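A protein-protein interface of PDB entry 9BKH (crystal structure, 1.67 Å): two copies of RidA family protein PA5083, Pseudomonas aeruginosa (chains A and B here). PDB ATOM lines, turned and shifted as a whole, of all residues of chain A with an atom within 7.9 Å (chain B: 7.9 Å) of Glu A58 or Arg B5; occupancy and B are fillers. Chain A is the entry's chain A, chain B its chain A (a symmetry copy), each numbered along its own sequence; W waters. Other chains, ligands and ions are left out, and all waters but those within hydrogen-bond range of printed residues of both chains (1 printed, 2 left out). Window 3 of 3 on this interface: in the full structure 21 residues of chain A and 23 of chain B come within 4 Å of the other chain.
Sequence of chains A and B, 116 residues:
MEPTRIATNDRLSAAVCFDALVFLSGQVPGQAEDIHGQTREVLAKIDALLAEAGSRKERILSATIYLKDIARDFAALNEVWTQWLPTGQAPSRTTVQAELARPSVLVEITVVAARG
CD of Pro B3 touches NH1 of Arg A59, at 3.7 Å.
Pro B3 touches Leu A61.
CE1 of Phe B23 touches CD1 of Leu A61, 3.7 Å away.
Gly A88 touches Thr B8.
C of Gln A89 touches NE of Arg B5 (3.5 Å).
Ala A90 touches Asn B9.
Val B16 touches Pro A91.
Ser A92 touches Ser B13.
Ser A92 touches Val B16 (N to CG2, 3.4 Å).
Phe B18 touches Ala A114 (CZ to CB, 3.5 Å).
Printed residues of chain B within 4 Å of Glu A58: Arg B5.
Printed residues of chain B within 4 Å of Leu A61: Pro B3 (3.9 Å), Val B16 (3.8 Å), Phe B18 (3.6 Å) and Phe B23 (3.7 Å).
Arg B5 touches just these residues of chain A: Glu A58 (2.8 Å), Gln A89 (3.5 Å) and Ala A90 (3.4 Å).
Of the printed residues of chain A, Thr B8 touches Gly A88 (3.6 Å).
Of the printed residues of chain A, Leu B12 touches Ala A90 and Pro A91.
The nearest residue of chain B that does not touch Glu A58 is Pro B3 (4.6 Å).
The nearest residue of chain A that does not touch Arg B5 is Gly A88 (4.4 Å).
The nearest printed residue of chain B that does not touch Gln A89 is Thr B8 (4.6 Å).
Water W1 lies within hydrogen-bond range of O of Ile A60 (2.6 Å), NH2 of Arg B5 (2.8 Å) and O of Gln A89 (3.2 Å).
No position is printed for both chains.
Of the 21 pairs that touch across the chains among the printed residues, none has its exchanged pair printed and touching as well.
The side-chain hydroxyl (OG) of Ser A55 sits at hydrogen-bond distance from the backbone carbonyl oxygen (O) of Ala A114, 2.7 Å away.
The guanidinium group (NE) of Arg A56 lies within salt-bridge range of the side-chain carboxylate (OE1) of Glu A58.
The side-chain hydroxyl of Ser A92 sits at hydrogen-bond distance from the backbone carbonyl oxygen of Leu A61, at 2.8 Å.
OE1 of Gln A89 lies close to O of Thr A87 (3.2 Å).
OG1 of Thr B8 is in hydrogen-bond range of OG of Ser B13, at 2.7 Å.
The side-chain amide oxygen of Asn B9 is in hydrogen-bond range of the backbone NH of Leu B12.
Of the 19 printed residues of chain A, 9 touch a printed residue of chain B.
Hydrophobic or aromatic side chains of chain A that line the printed part of chain B: Leu A61, Ala A90 and Ala A114.
Printed residues of chain B that touch a printed residue of chain A: Glu B2, Pro B3, Arg B5, Thr B8, Asn B9, Leu B12, Ser B13, Val B16, Phe B18 and Phe B23.
Hydrophobic or aromatic side chains of chain B within 4 Å of the printed part of chain A: Pro B3, Leu B12, Val B16, Phe B18 and Phe B23.
Along chain B the printed residues that touch a printed residue of chain A span positions 2 to 23.
Among the printed residues, 21 pairs touch across the chains.
Among the printed residues, no Asp or Glu carboxylate lies within 4 Å of a Lys or Arg side-chain nitrogen of the other chain.
O of Glu A58 sits at hydrogen-bond distance from NH2 of Arg B5 (2.8 Å).
The guanidinium group (NE) of Arg B5 sits close to the backbone carbonyl oxygen (O) of Ala A90, at 3.4 Å.
The backbone carbonyl oxygen (O) of Ala A90 sits at hydrogen-bond distance from the side-chain hydroxyl (OG) of Ser B13 (2.8 Å).
The backbone carbonyl oxygen (O) of Pro A91 sits at hydrogen-bond distance from the backbone NH (N) of Ser B13 (2.9 Å).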
ATOM      1  N   LEU A  50     -10.572  30.346  -0.751  1.00  0.00           N
ATOM      2  CA  LEU A  50      -9.594  29.503  -0.080  1.00  0.00           C
ATOM      3  C   LEU A  50      -8.395  30.337   0.361  1.00  0.00           C
ATOM      4  O   LEU A  50      -7.946  30.236   1.510  1.00  0.00           O
ATOM      5  CB  LEU A  50      -9.130  28.373  -0.980  1.00  0.00           C
ATOM      6  CG  LEU A  50     -10.193  27.336  -1.329  1.00  0.00           C
ATOM      7  CD1 LEU A  50      -9.645  26.323  -2.314  1.00  0.00           C
ATOM      8  CD2 LEU A  50     -10.684  26.620  -0.050  1.00  0.00           C
ATOM      9  N   SER A  55      -6.402  28.702   3.284  1.00  0.00           N
ATOM     10  CA  SER A  55      -6.294  27.389   2.665  1.00  0.00           C
ATOM     11  C   SER A  55      -5.747  27.508   1.253  1.00  0.00           C
ATOM     12  O   SER A  55      -5.182  28.559   0.889  1.00  0.00           O
ATOM     13  CB  SER A  55      -7.682  26.717   2.646  1.00  0.00           C
ATOM     14  OG  SER A  55      -7.573  25.351   2.294  1.00  0.00           O
ATOM     15  N   ARG A  56      -5.899  26.472   0.448  1.00  0.00           N
ATOM     16  CA  ARG A  56      -5.432  26.475  -0.933  1.00  0.00           C
ATOM     17  C   ARG A  56      -6.061  25.282  -1.647  1.00  0.00           C
ATOM     18  O   ARG A  56      -6.616  24.379  -1.012  1.00  0.00           O
ATOM     19  CB  ARG A  56      -3.906  26.424  -1.002  1.00  0.00           C
ATOM     20  CG  ARG A  56      -3.309  25.255  -0.274  1.00  0.00           C
ATOM     21  CD  ARG A  56      -1.784  25.341  -0.196  1.00  0.00           C
ATOM     22  NE  ARG A  56      -1.169  25.373  -1.513  1.00  0.00           N
ATOM     23  CZ  ARG A  56       0.139  25.469  -1.719  1.00  0.00           C
ATOM     24  NH1 ARG A  56       0.991  25.493  -0.708  1.00  0.00           N
ATOM     25  NH2 ARG A  56       0.597  25.544  -2.968  1.00  0.00           N
ATOM     26  N   LYS A  57      -5.933  25.268  -2.971  1.00  0.00           N
ATOM     27  CA  LYS A  57      -6.582  24.213  -3.754  1.00  0.00           C
ATOM     28  C   LYS A  57      -6.103  22.825  -3.344  1.00  0.00           C
ATOM     29  O   LYS A  57      -6.894  21.871  -3.343  1.00  0.00           O
ATOM     30  CB  LYS A  57      -6.341  24.412  -5.258  1.00  0.00           C
ATOM     31  CG  LYS A  57      -6.779  25.764  -5.796  1.00  0.00           C
ATOM     32  CD  LYS A  57      -6.980  25.750  -7.325  1.00  0.00           C
ATOM     33  CE  LYS A  57      -5.698  25.815  -8.105  1.00  0.00           C
ATOM     34  NZ  LYS A  57      -5.988  26.057  -9.543  1.00  0.00           N
ATOM     35  N   GLU A  58      -4.823  22.687  -2.961  1.00  0.00           N
ATOM     36  CA  GLU A  58      -4.283  21.403  -2.560  1.00  0.00           C
ATOM     37  C   GLU A  58      -4.843  20.891  -1.239  1.00  0.00           C
ATOM     38  O   GLU A  58      -4.548  19.754  -0.857  1.00  0.00           O
ATOM     39  CB  GLU A  58      -2.753  21.504  -2.453  1.00  0.00           C
ATOM     40  CG  GLU A  58      -2.065  21.815  -3.762  1.00  0.00           C
ATOM     41  CD  GLU A  58      -2.021  23.295  -4.128  1.00  0.00           C
ATOM     42  OE1 GLU A  58      -2.715  24.152  -3.514  1.00  0.00           O
ATOM     43  OE2 GLU A  58      -1.289  23.619  -5.087  1.00  0.00           O
ATOM     44  N   ARG A  59      -5.605  21.708  -0.518  1.00  0.00           N
ATOM     45  CA  ARG A  59      -6.150  21.330   0.778  1.00  0.00           C
ATOM     46  C   ARG A  59      -7.670  21.216   0.750  1.00  0.00           C
ATOM     47  O   ARG A  59      -8.306  21.179   1.801  1.00  0.00           O
ATOM     48  CB  ARG A  59      -5.684  22.316   1.846  1.00  0.00           C
ATOM     49  CG  ARG A  59      -4.154  22.282   2.042  1.00  0.00           C
ATOM     50  CD  ARG A  59      -3.670  23.235   3.126  1.00  0.00           C
ATOM     51  NE  ARG A  59      -3.940  22.740   4.469  1.00  0.00           N
ATOM     52  CZ  ARG A  59      -3.220  21.814   5.100  1.00  0.00           C
ATOM     53  NH1 ARG A  59      -2.199  21.212   4.514  1.00  0.00           N
ATOM     54  NH2 ARG A  59      -3.547  21.480   6.340  1.00  0.00           N
ATOM     55  N   ILE A  60      -8.265  21.130  -0.437  1.00  0.00           N
ATOM     56  CA  ILE A  60      -9.703  20.880  -0.504  1.00  0.00           C
ATOM     57  C   ILE A  60      -9.978  19.471   0.010  1.00  0.00           C
ATOM     58  O   ILE A  60      -9.279  18.507  -0.351  1.00  0.00           O
ATOM     59  CB  ILE A  60     -10.221  21.078  -1.933  1.00  0.00           C
ATOM     60  CG1 ILE A  60     -10.007  22.519  -2.395  1.00  0.00           C
ATOM     61  CG2 ILE A  60     -11.716  20.736  -1.994  1.00  0.00           C
ATOM     62  CD1 ILE A  60     -10.234  22.721  -3.893  1.00  0.00           C
ATOM     63  N   LEU A  61     -11.008  19.339   0.844  1.00  0.00           N
ATOM     64  CA  LEU A  61     -11.407  18.058   1.405  1.00  0.00           C
ATOM     65  C   LEU A  61     -12.591  17.454   0.664  1.00  0.00           C
ATOM     66  O   LEU A  61     -12.595  16.247   0.364  1.00  0.00           O
ATOM     67  CB  LEU A  61     -11.738  18.223   2.891  1.00  0.00           C
ATOM     68  CG  LEU A  61     -10.580  18.756   3.755  1.00  0.00           C
ATOM     69  CD1 LEU A  61     -11.074  18.978   5.161  1.00  0.00           C
ATOM     70  CD2 LEU A  61      -9.398  17.831   3.735  1.00  0.00           C
ATOM     71  N   TRP A  84      -8.283  22.709 -13.602  1.00  0.00           N
ATOM     72  CA  TRP A  84      -8.115  23.630 -12.480  1.00  0.00           C
ATOM     73  C   TRP A  84      -7.457  22.957 -11.296  1.00  0.00           C
ATOM     74  O   TRP A  84      -6.762  23.626 -10.511  1.00  0.00           O
ATOM     75  CB  TRP A  84      -9.479  24.180 -12.088  1.00  0.00           C
ATOM     76  CG  TRP A  84      -9.545  25.112 -10.915  1.00  0.00           C
ATOM     77  CD1 TRP A  84      -9.322  26.461 -10.913  1.00  0.00           C
ATOM     78  CD2 TRP A  84      -9.948  24.778  -9.581  1.00  0.00           C
ATOM     79  NE1 TRP A  84      -9.541  26.983  -9.665  1.00  0.00           N
ATOM     80  CE2 TRP A  84      -9.927  25.968  -8.826  1.00  0.00           C
ATOM     81  CE3 TRP A  84     -10.334  23.589  -8.956  1.00  0.00           C
ATOM     82  CZ2 TRP A  84     -10.287  26.002  -7.483  1.00  0.00           C
ATOM     83  CZ3 TRP A  84     -10.662  23.622  -7.621  1.00  0.00           C
ATOM     84  CH2 TRP A  84     -10.620  24.810  -6.894  1.00  0.00           C
ATOM     85  N   LEU A  85      -7.652  21.650 -11.137  1.00  0.00           N
ATOM     86  CA  LEU A  85      -7.170  20.979  -9.943  1.00  0.00           C
ATOM     87  C   LEU A  85      -5.651  20.871  -9.927  1.00  0.00           C
ATOM     88  O   LEU A  85      -5.014  20.668 -10.965  1.00  0.00           O
ATOM     89  CB  LEU A  85      -7.741  19.570  -9.843  1.00  0.00           C
ATOM     90  CG  LEU A  85      -9.183  19.390  -9.357  1.00  0.00           C
ATOM     91  CD1 LEU A  85      -9.533  17.902  -9.333  1.00  0.00           C
ATOM     92  CD2 LEU A  85      -9.385  20.039  -7.990  1.00  0.00           C
ATOM     93  N   PRO A  86      -5.047  20.935  -8.751  1.00  0.00           N
ATOM     94  CA  PRO A  86      -3.622  20.608  -8.645  1.00  0.00           C
ATOM     95  C   PRO A  86      -3.362  19.140  -8.968  1.00  0.00           C
ATOM     96  O   PRO A  86      -4.071  18.240  -8.508  1.00  0.00           O
ATOM     97  CB  PRO A  86      -3.278  20.942  -7.187  1.00  0.00           C
ATOM     98  CG  PRO A  86      -4.596  20.860  -6.452  1.00  0.00           C
ATOM     99  CD  PRO A  86      -5.679  21.189  -7.438  1.00  0.00           C
ATOM    100  N   THR A  87      -2.316  18.901  -9.760  1.00  0.00           N
ATOM    101  CA  THR A  87      -2.078  17.562 -10.290  1.00  0.00           C
ATOM    102  C   THR A  87      -1.949  16.538  -9.177  1.00  0.00           C
ATOM    103  O   THR A  87      -1.238  16.757  -8.188  1.00  0.00           O
ATOM    104  CB  THR A  87      -0.812  17.548 -11.158  1.00  0.00           C
ATOM    105  OG1 THR A  87      -0.958  18.467 -12.247  1.00  0.00           O
ATOM    106  CG2 THR A  87      -0.558  16.146 -11.708  1.00  0.00           C
ATOM    107  N   GLY A  88      -2.642  15.410  -9.345  1.00  0.00           N
ATOM    108  CA  GLY A  88      -2.600  14.317  -8.407  1.00  0.00           C
ATOM    109  C   GLY A  88      -3.219  14.585  -7.062  1.00  0.00           C
ATOM    110  O   GLY A  88      -3.092  13.750  -6.164  1.00  0.00           O
ATOM    111  N   GLN A  89      -3.890  15.722  -6.882  1.00  0.00           N
ATOM    112  CA  GLN A  89      -4.374  16.131  -5.575  1.00  0.00           C
ATOM    113  C   GLN A  89      -5.866  16.458  -5.591  1.00  0.00           C
ATOM    114  O   GLN A  89      -6.317  17.413  -4.954  1.00  0.00           O
ATOM    115  CB  GLN A  89      -3.568  17.318  -5.064  1.00  0.00           C
ATOM    116  CG  GLN A  89      -2.122  16.946  -4.797  1.00  0.00           C
ATOM    117  CD  GLN A  89      -1.234  18.156  -4.689  1.00  0.00           C
ATOM    118  OE1 GLN A  89      -0.801  18.713  -5.696  1.00  0.00           O
ATOM    119  NE2 GLN A  89      -0.968  18.573  -3.478  1.00  0.00           N
ATOM    120  N   ALA A  90      -6.660  15.654  -6.282  1.00  0.00           N
ATOM    121  CA  ALA A  90      -8.088  15.917  -6.353  1.00  0.00           C
ATOM    122  C   ALA A  90      -8.773  15.615  -5.021  1.00  0.00           C
ATOM    123  O   ALA A  90      -8.382  14.694  -4.296  1.00  0.00           O
ATOM    124  CB  ALA A  90      -8.722  15.082  -7.454  1.00  0.00           C
ATOM    125  N   PRO A  91      -9.844  16.349  -4.701  1.00  0.00           N
ATOM    126  CA  PRO A  91     -10.550  16.123  -3.434  1.00  0.00           C
ATOM    127  C   PRO A  91     -11.617  15.044  -3.542  1.00  0.00           C
ATOM    128  O   PRO A  91     -11.848  14.505  -4.625  1.00  0.00           O
ATOM    129  CB  PRO A  91     -11.180  17.505  -3.161  1.00  0.00           C
ATOM    130  CG  PRO A  91     -11.547  17.983  -4.556  1.00  0.00           C
ATOM    131  CD  PRO A  91     -10.402  17.486  -5.455  1.00  0.00           C
ATOM    132  N   SER A  92     -12.306  14.729  -2.450  1.00  0.00           N
ATOM    133  CA  SER A  92     -13.546  13.978  -2.596  1.00  0.00           C
ATOM    134  C   SER A  92     -14.572  14.857  -3.311  1.00  0.00           C
ATOM    135  O   SER A  92     -14.572  16.082  -3.189  1.00  0.00           O
ATOM    136  CB  SER A  92     -14.069  13.483  -1.244  1.00  0.00           C
ATOM    137  OG  SER A  92     -14.609  14.496  -0.436  1.00  0.00           O
ATOM    138  N   ALA A 113     -12.644  22.707   3.076  1.00  0.00           N
ATOM    139  CA  ALA A 113     -11.204  22.580   2.909  1.00  0.00           C
ATOM    140  C   ALA A 113     -10.514  22.655   4.271  1.00  0.00           C
ATOM    141  O   ALA A 113     -11.116  23.038   5.277  1.00  0.00           O
ATOM    142  CB  ALA A 113     -10.643  23.680   1.991  1.00  0.00           C
ATOM    143  N   ALA A 114      -9.236  22.316   4.278  1.00  0.00           N
ATOM    144  CA  ALA A 114      -8.407  22.348   5.478  1.00  0.00           C
ATOM    145  C   ALA A 114      -7.555  23.607   5.498  1.00  0.00           C
ATOM    146  O   ALA A 114      -6.901  23.934   4.503  1.00  0.00           O
ATOM    147  CB  ALA A 114      -7.492  21.135   5.548  1.00  0.00           C
ATOM    148  N   GLU B   2      -1.488  17.444   7.019  1.00  0.00           N
ATOM    149  CA  GLU B   2      -1.924  17.495   5.633  1.00  0.00           C
ATOM    150  C   GLU B   2      -3.017  16.472   5.355  1.00  0.00           C
ATOM    151  O   GLU B   2      -3.026  15.386   5.939  1.00  0.00           O
ATOM    152  CB  GLU B   2      -0.759  17.234   4.667  1.00  0.00           C
ATOM    153  CG  GLU B   2       0.022  18.480   4.257  1.00  0.00           C
ATOM    154  CD  GLU B   2       0.820  18.269   2.980  1.00  0.00           C
ATOM    155  OE1 GLU B   2       0.904  19.216   2.166  1.00  0.00           O
ATOM    156  OE2 GLU B   2       1.349  17.152   2.785  1.00  0.00           O
ATOM    157  N   PRO B   3      -3.947  16.795   4.455  1.00  0.00           N
ATOM    158  CA  PRO B   3      -4.883  15.774   3.964  1.00  0.00           C
ATOM    159  C   PRO B   3      -4.139  14.641   3.275  1.00  0.00           C
ATOM    160  O   PRO B   3      -3.118  14.846   2.610  1.00  0.00           O
ATOM    161  CB  PRO B   3      -5.757  16.538   2.965  1.00  0.00           C
ATOM    162  CG  PRO B   3      -5.546  17.973   3.256  1.00  0.00           C
ATOM    163  CD  PRO B   3      -4.173  18.103   3.821  1.00  0.00           C
ATOM    164  N   THR B   4      -4.673  13.436   3.411  1.00  0.00           N
ATOM    165  CA  THR B   4      -4.199  12.289   2.656  1.00  0.00           C
ATOM    166  C   THR B   4      -5.355  11.732   1.837  1.00  0.00           C
ATOM    167  O   THR B   4      -6.532  11.953   2.150  1.00  0.00           O
ATOM    168  CB  THR B   4      -3.623  11.226   3.574  1.00  0.00           C
ATOM    169  OG1 THR B   4      -4.633  10.760   4.462  1.00  0.00           O
ATOM    170  CG2 THR B   4      -2.452  11.818   4.381  1.00  0.00           C
ATOM    171  N   ARG B   5      -5.014  11.030   0.765  1.00  0.00           N
ATOM    172  CA  ARG B   5      -6.011  10.653  -0.226  1.00  0.00           C
ATOM    173  C   ARG B   5      -5.936   9.172  -0.538  1.00  0.00           C
ATOM    174  O   ARG B   5      -4.864   8.565  -0.506  1.00  0.00           O
ATOM    175  CB  ARG B   5      -5.844  11.467  -1.510  1.00  0.00           C
ATOM    176  CG  ARG B   5      -5.776  12.952  -1.281  1.00  0.00           C
ATOM    177  CD  ARG B   5      -5.632  13.702  -2.576  1.00  0.00           C
ATOM    178  NE  ARG B   5      -5.639  15.133  -2.329  1.00  0.00           N
ATOM    179  CZ  ARG B   5      -4.597  15.840  -1.929  1.00  0.00           C
ATOM    180  NH1 ARG B   5      -3.409  15.281  -1.758  1.00  0.00           N
ATOM    181  NH2 ARG B   5      -4.748  17.136  -1.699  1.00  0.00           N
ATOM    182  N   ILE B   6      -7.101   8.595  -0.838  1.00  0.00           N
ATOM    183  CA  ILE B   6      -7.246   7.202  -1.236  1.00  0.00           C
ATOM    184  C   ILE B   6      -7.934   7.161  -2.599  1.00  0.00           C
ATOM    185  O   ILE B   6      -8.991   7.774  -2.787  1.00  0.00           O
ATOM    186  CB  ILE B   6      -8.053   6.420  -0.189  1.00  0.00           C
ATOM    187  CG1 ILE B   6      -7.288   6.310   1.134  1.00  0.00           C
ATOM    188  CG2 ILE B   6      -8.427   5.014  -0.691  1.00  0.00           C
ATOM    189  CD1 ILE B   6      -8.197   6.002   2.329  1.00  0.00           C
ATOM    190  N   ALA B   7      -7.314   6.466  -3.559  1.00  0.00           N
ATOM    191  CA  ALA B   7      -7.889   6.198  -4.878  1.00  0.00           C
ATOM    192  C   ALA B   7      -8.179   7.491  -5.651  1.00  0.00           C
ATOM    193  O   ALA B   7      -9.321   7.862  -5.931  1.00  0.00           O
ATOM    194  CB  ALA B   7      -9.142   5.328  -4.727  1.00  0.00           C
ATOM    195  N   THR B   8      -7.085   8.124  -6.055  1.00  0.00           N
ATOM    196  CA  THR B   8      -7.110   9.408  -6.735  1.00  0.00           C
ATOM    197  C   THR B   8      -7.058   9.225  -8.247  1.00  0.00           C
ATOM    198  O   THR B   8      -6.230   8.463  -8.756  1.00  0.00           O
ATOM    199  CB  THR B   8      -5.917  10.265  -6.277  1.00  0.00           C
ATOM    200  OG1 THR B   8      -5.953  10.445  -4.856  1.00  0.00           O
ATOM    201  CG2 THR B   8      -5.907  11.604  -6.983  1.00  0.00           C
ATOM    202  N   ASN B   9      -7.945   9.918  -8.957  1.00  0.00           N
ATOM    203  CA  ASN B   9      -7.858  10.034 -10.409  1.00  0.00           C
ATOM    204  C   ASN B   9      -7.898  11.516 -10.771  1.00  0.00           C
ATOM    205  O   ASN B   9      -7.767  12.383  -9.889  1.00  0.00           O
ATOM    206  CB  ASN B   9      -8.971   9.208 -11.080  1.00  0.00           C
ATOM    207  CG  ASN B   9     -10.378   9.682 -10.718  1.00  0.00           C
ATOM    208  OD1 ASN B   9     -10.660  10.868 -10.704  1.00  0.00           O
ATOM    209  ND2 ASN B   9     -11.267   8.736 -10.439  1.00  0.00           N
ATOM    210  N   LEU B  12     -11.250  13.136  -8.891  1.00  0.00           N
ATOM    211  CA  LEU B  12     -11.614  12.981  -7.490  1.00  0.00           C
ATOM    212  C   LEU B  12     -10.701  11.968  -6.819  1.00  0.00           C
ATOM    213  O   LEU B  12     -10.016  11.183  -7.476  1.00  0.00           O
ATOM    214  CB  LEU B  12     -13.078  12.550  -7.351  1.00  0.00           C
ATOM    215  CG  LEU B  12     -13.513  11.254  -8.044  1.00  0.00           C
ATOM    216  CD1 LEU B  12     -13.191  10.028  -7.251  1.00  0.00           C
ATOM    217  CD2 LEU B  12     -15.021  11.312  -8.287  1.00  0.00           C
ATOM    218  N   SER B  13     -10.730  11.982  -5.492  1.00  0.00           N
ATOM    219  CA  SER B  13     -10.238  10.889  -4.668  1.00  0.00           C
ATOM    220  C   SER B  13     -11.433  10.233  -3.990  1.00  0.00           C
ATOM    221  O   SER B  13     -12.326  10.921  -3.462  1.00  0.00           O
ATOM    222  CB  SER B  13      -9.238  11.353  -3.616  1.00  0.00           C
ATOM    223  OG  SER B  13      -8.118  11.940  -4.230  1.00  0.00           O
ATOM    224  N   ALA B  14     -11.433   8.895  -3.983  1.00  0.00           N
ATOM    225  CA  ALA B  14     -12.533   8.170  -3.364  1.00  0.00           C
ATOM    226  C   ALA B  14     -12.706   8.570  -1.909  1.00  0.00           C
ATOM    227  O   ALA B  14     -13.832   8.616  -1.411  1.00  0.00           O
ATOM    228  CB  ALA B  14     -12.312   6.657  -3.478  1.00  0.00           C
ATOM    229  N   ALA B  15     -11.596   8.819  -1.193  1.00  0.00           N
ATOM    230  CA  ALA B  15     -11.637   9.293   0.175  1.00  0.00           C
ATOM    231  C   ALA B  15     -10.503  10.285   0.379  1.00  0.00           C
ATOM    232  O   ALA B  15      -9.428  10.139  -0.207  1.00  0.00           O
ATOM    233  CB  ALA B  15     -11.501   8.164   1.193  1.00  0.00           C
ATOM    234  N   VAL B  16     -10.784  11.320   1.159  1.00  0.00           N
ATOM    235  CA  VAL B  16      -9.774  12.243   1.666  1.00  0.00           C
ATOM    236  C   VAL B  16      -9.860  12.230   3.182  1.00  0.00           C
ATOM    237  O   VAL B  16     -10.940  12.418   3.757  1.00  0.00           O
ATOM    238  CB  VAL B  16      -9.963  13.667   1.114  1.00  0.00           C
ATOM    239  CG1 VAL B  16      -8.940  14.600   1.731  1.00  0.00           C
ATOM    240  CG2 VAL B  16      -9.837  13.685  -0.390  1.00  0.00           C
ATOM    241  N   CYS B  17      -8.725  12.006   3.830  1.00  0.00           N
ATOM    242  CA  CYS B  17      -8.638  11.999   5.277  1.00  0.00           C
ATOM    243  C   CYS B  17      -7.952  13.267   5.763  1.00  0.00           C
ATOM    244  O   CYS B  17      -6.974  13.720   5.165  1.00  0.00           O
ATOM    245  CB  CYS B  17      -7.870  10.775   5.768  1.00  0.00           C
ATOM    246  SG  CYS B  17      -8.608   9.218   5.175  1.00  0.00           S
ATOM    247  N   PHE B  18      -8.486  13.850   6.830  1.00  0.00           N
ATOM    248  CA  PHE B  18      -7.855  15.030   7.423  1.00  0.00           C
ATOM    249  C   PHE B  18      -8.079  14.963   8.922  1.00  0.00           C
ATOM    250  O   PHE B  18      -9.221  15.018   9.390  1.00  0.00           O
ATOM    251  CB  PHE B  18      -8.385  16.340   6.843  1.00  0.00           C
ATOM    252  CG  PHE B  18      -7.710  17.546   7.431  1.00  0.00           C
ATOM    253  CD1 PHE B  18      -6.346  17.733   7.266  1.00  0.00           C
ATOM    254  CD2 PHE B  18      -8.421  18.443   8.189  1.00  0.00           C
ATOM    255  CE1 PHE B  18      -5.710  18.821   7.846  1.00  0.00           C
ATOM    256  CE2 PHE B  18      -7.784  19.523   8.772  1.00  0.00           C
ATOM    257  CZ  PHE B  18      -6.429  19.704   8.594  1.00  0.00           C
ATOM    258  N   PHE B  23     -13.662  12.055   4.466  1.00  0.00           N
ATOM    259  CA  PHE B  23     -14.615  12.553   3.475  1.00  0.00           C
ATOM    260  C   PHE B  23     -14.626  11.611   2.279  1.00  0.00           C
ATOM    261  O   PHE B  23     -13.623  11.486   1.573  1.00  0.00           O
ATOM    262  CB  PHE B  23     -14.240  13.971   3.009  1.00  0.00           C
ATOM    263  CG  PHE B  23     -14.231  14.979   4.107  1.00  0.00           C
ATOM    264  CD1 PHE B  23     -13.160  15.055   4.996  1.00  0.00           C
ATOM    265  CD2 PHE B  23     -15.286  15.863   4.260  1.00  0.00           C
ATOM    266  CE1 PHE B  23     -13.165  16.004   6.041  1.00  0.00           C
ATOM    267  CE2 PHE B  23     -15.293  16.802   5.297  1.00  0.00           C
ATOM    268  CZ  PHE B  23     -14.222  16.870   6.184  1.00  0.00           C
ATOM    269  N   ARG B 115     -12.469   8.982  11.893  1.00  0.00           N
ATOM    270  CA  ARG B 115     -11.417   7.982  12.012  1.00  0.00           C
ATOM    271  C   ARG B 115     -11.494   7.323  13.379  1.00  0.00           C
ATOM    272  O   ARG B 115     -11.964   7.918  14.351  1.00  0.00           O
ATOM    273  CB  ARG B 115     -10.045   8.625  11.843  1.00  0.00           C
ATOM    274  CG  ARG B 115      -9.747   9.074  10.443  1.00  0.00           C
ATOM    275  CD  ARG B 115      -8.999   7.996   9.680  1.00  0.00           C
ATOM    276  NE  ARG B 115      -8.003   8.581   8.792  1.00  0.00           N
ATOM    277  CZ  ARG B 115      -6.691   8.517   8.987  1.00  0.00           C
ATOM    278  NH1 ARG B 115      -6.168   7.740   9.924  1.00  0.00           N
ATOM    279  NH2 ARG B 115      -5.887   9.250   8.222  1.00  0.00           N
HETATM  280  O   HOH W   1      -7.533  17.471  -2.019  1.00  0.00           O
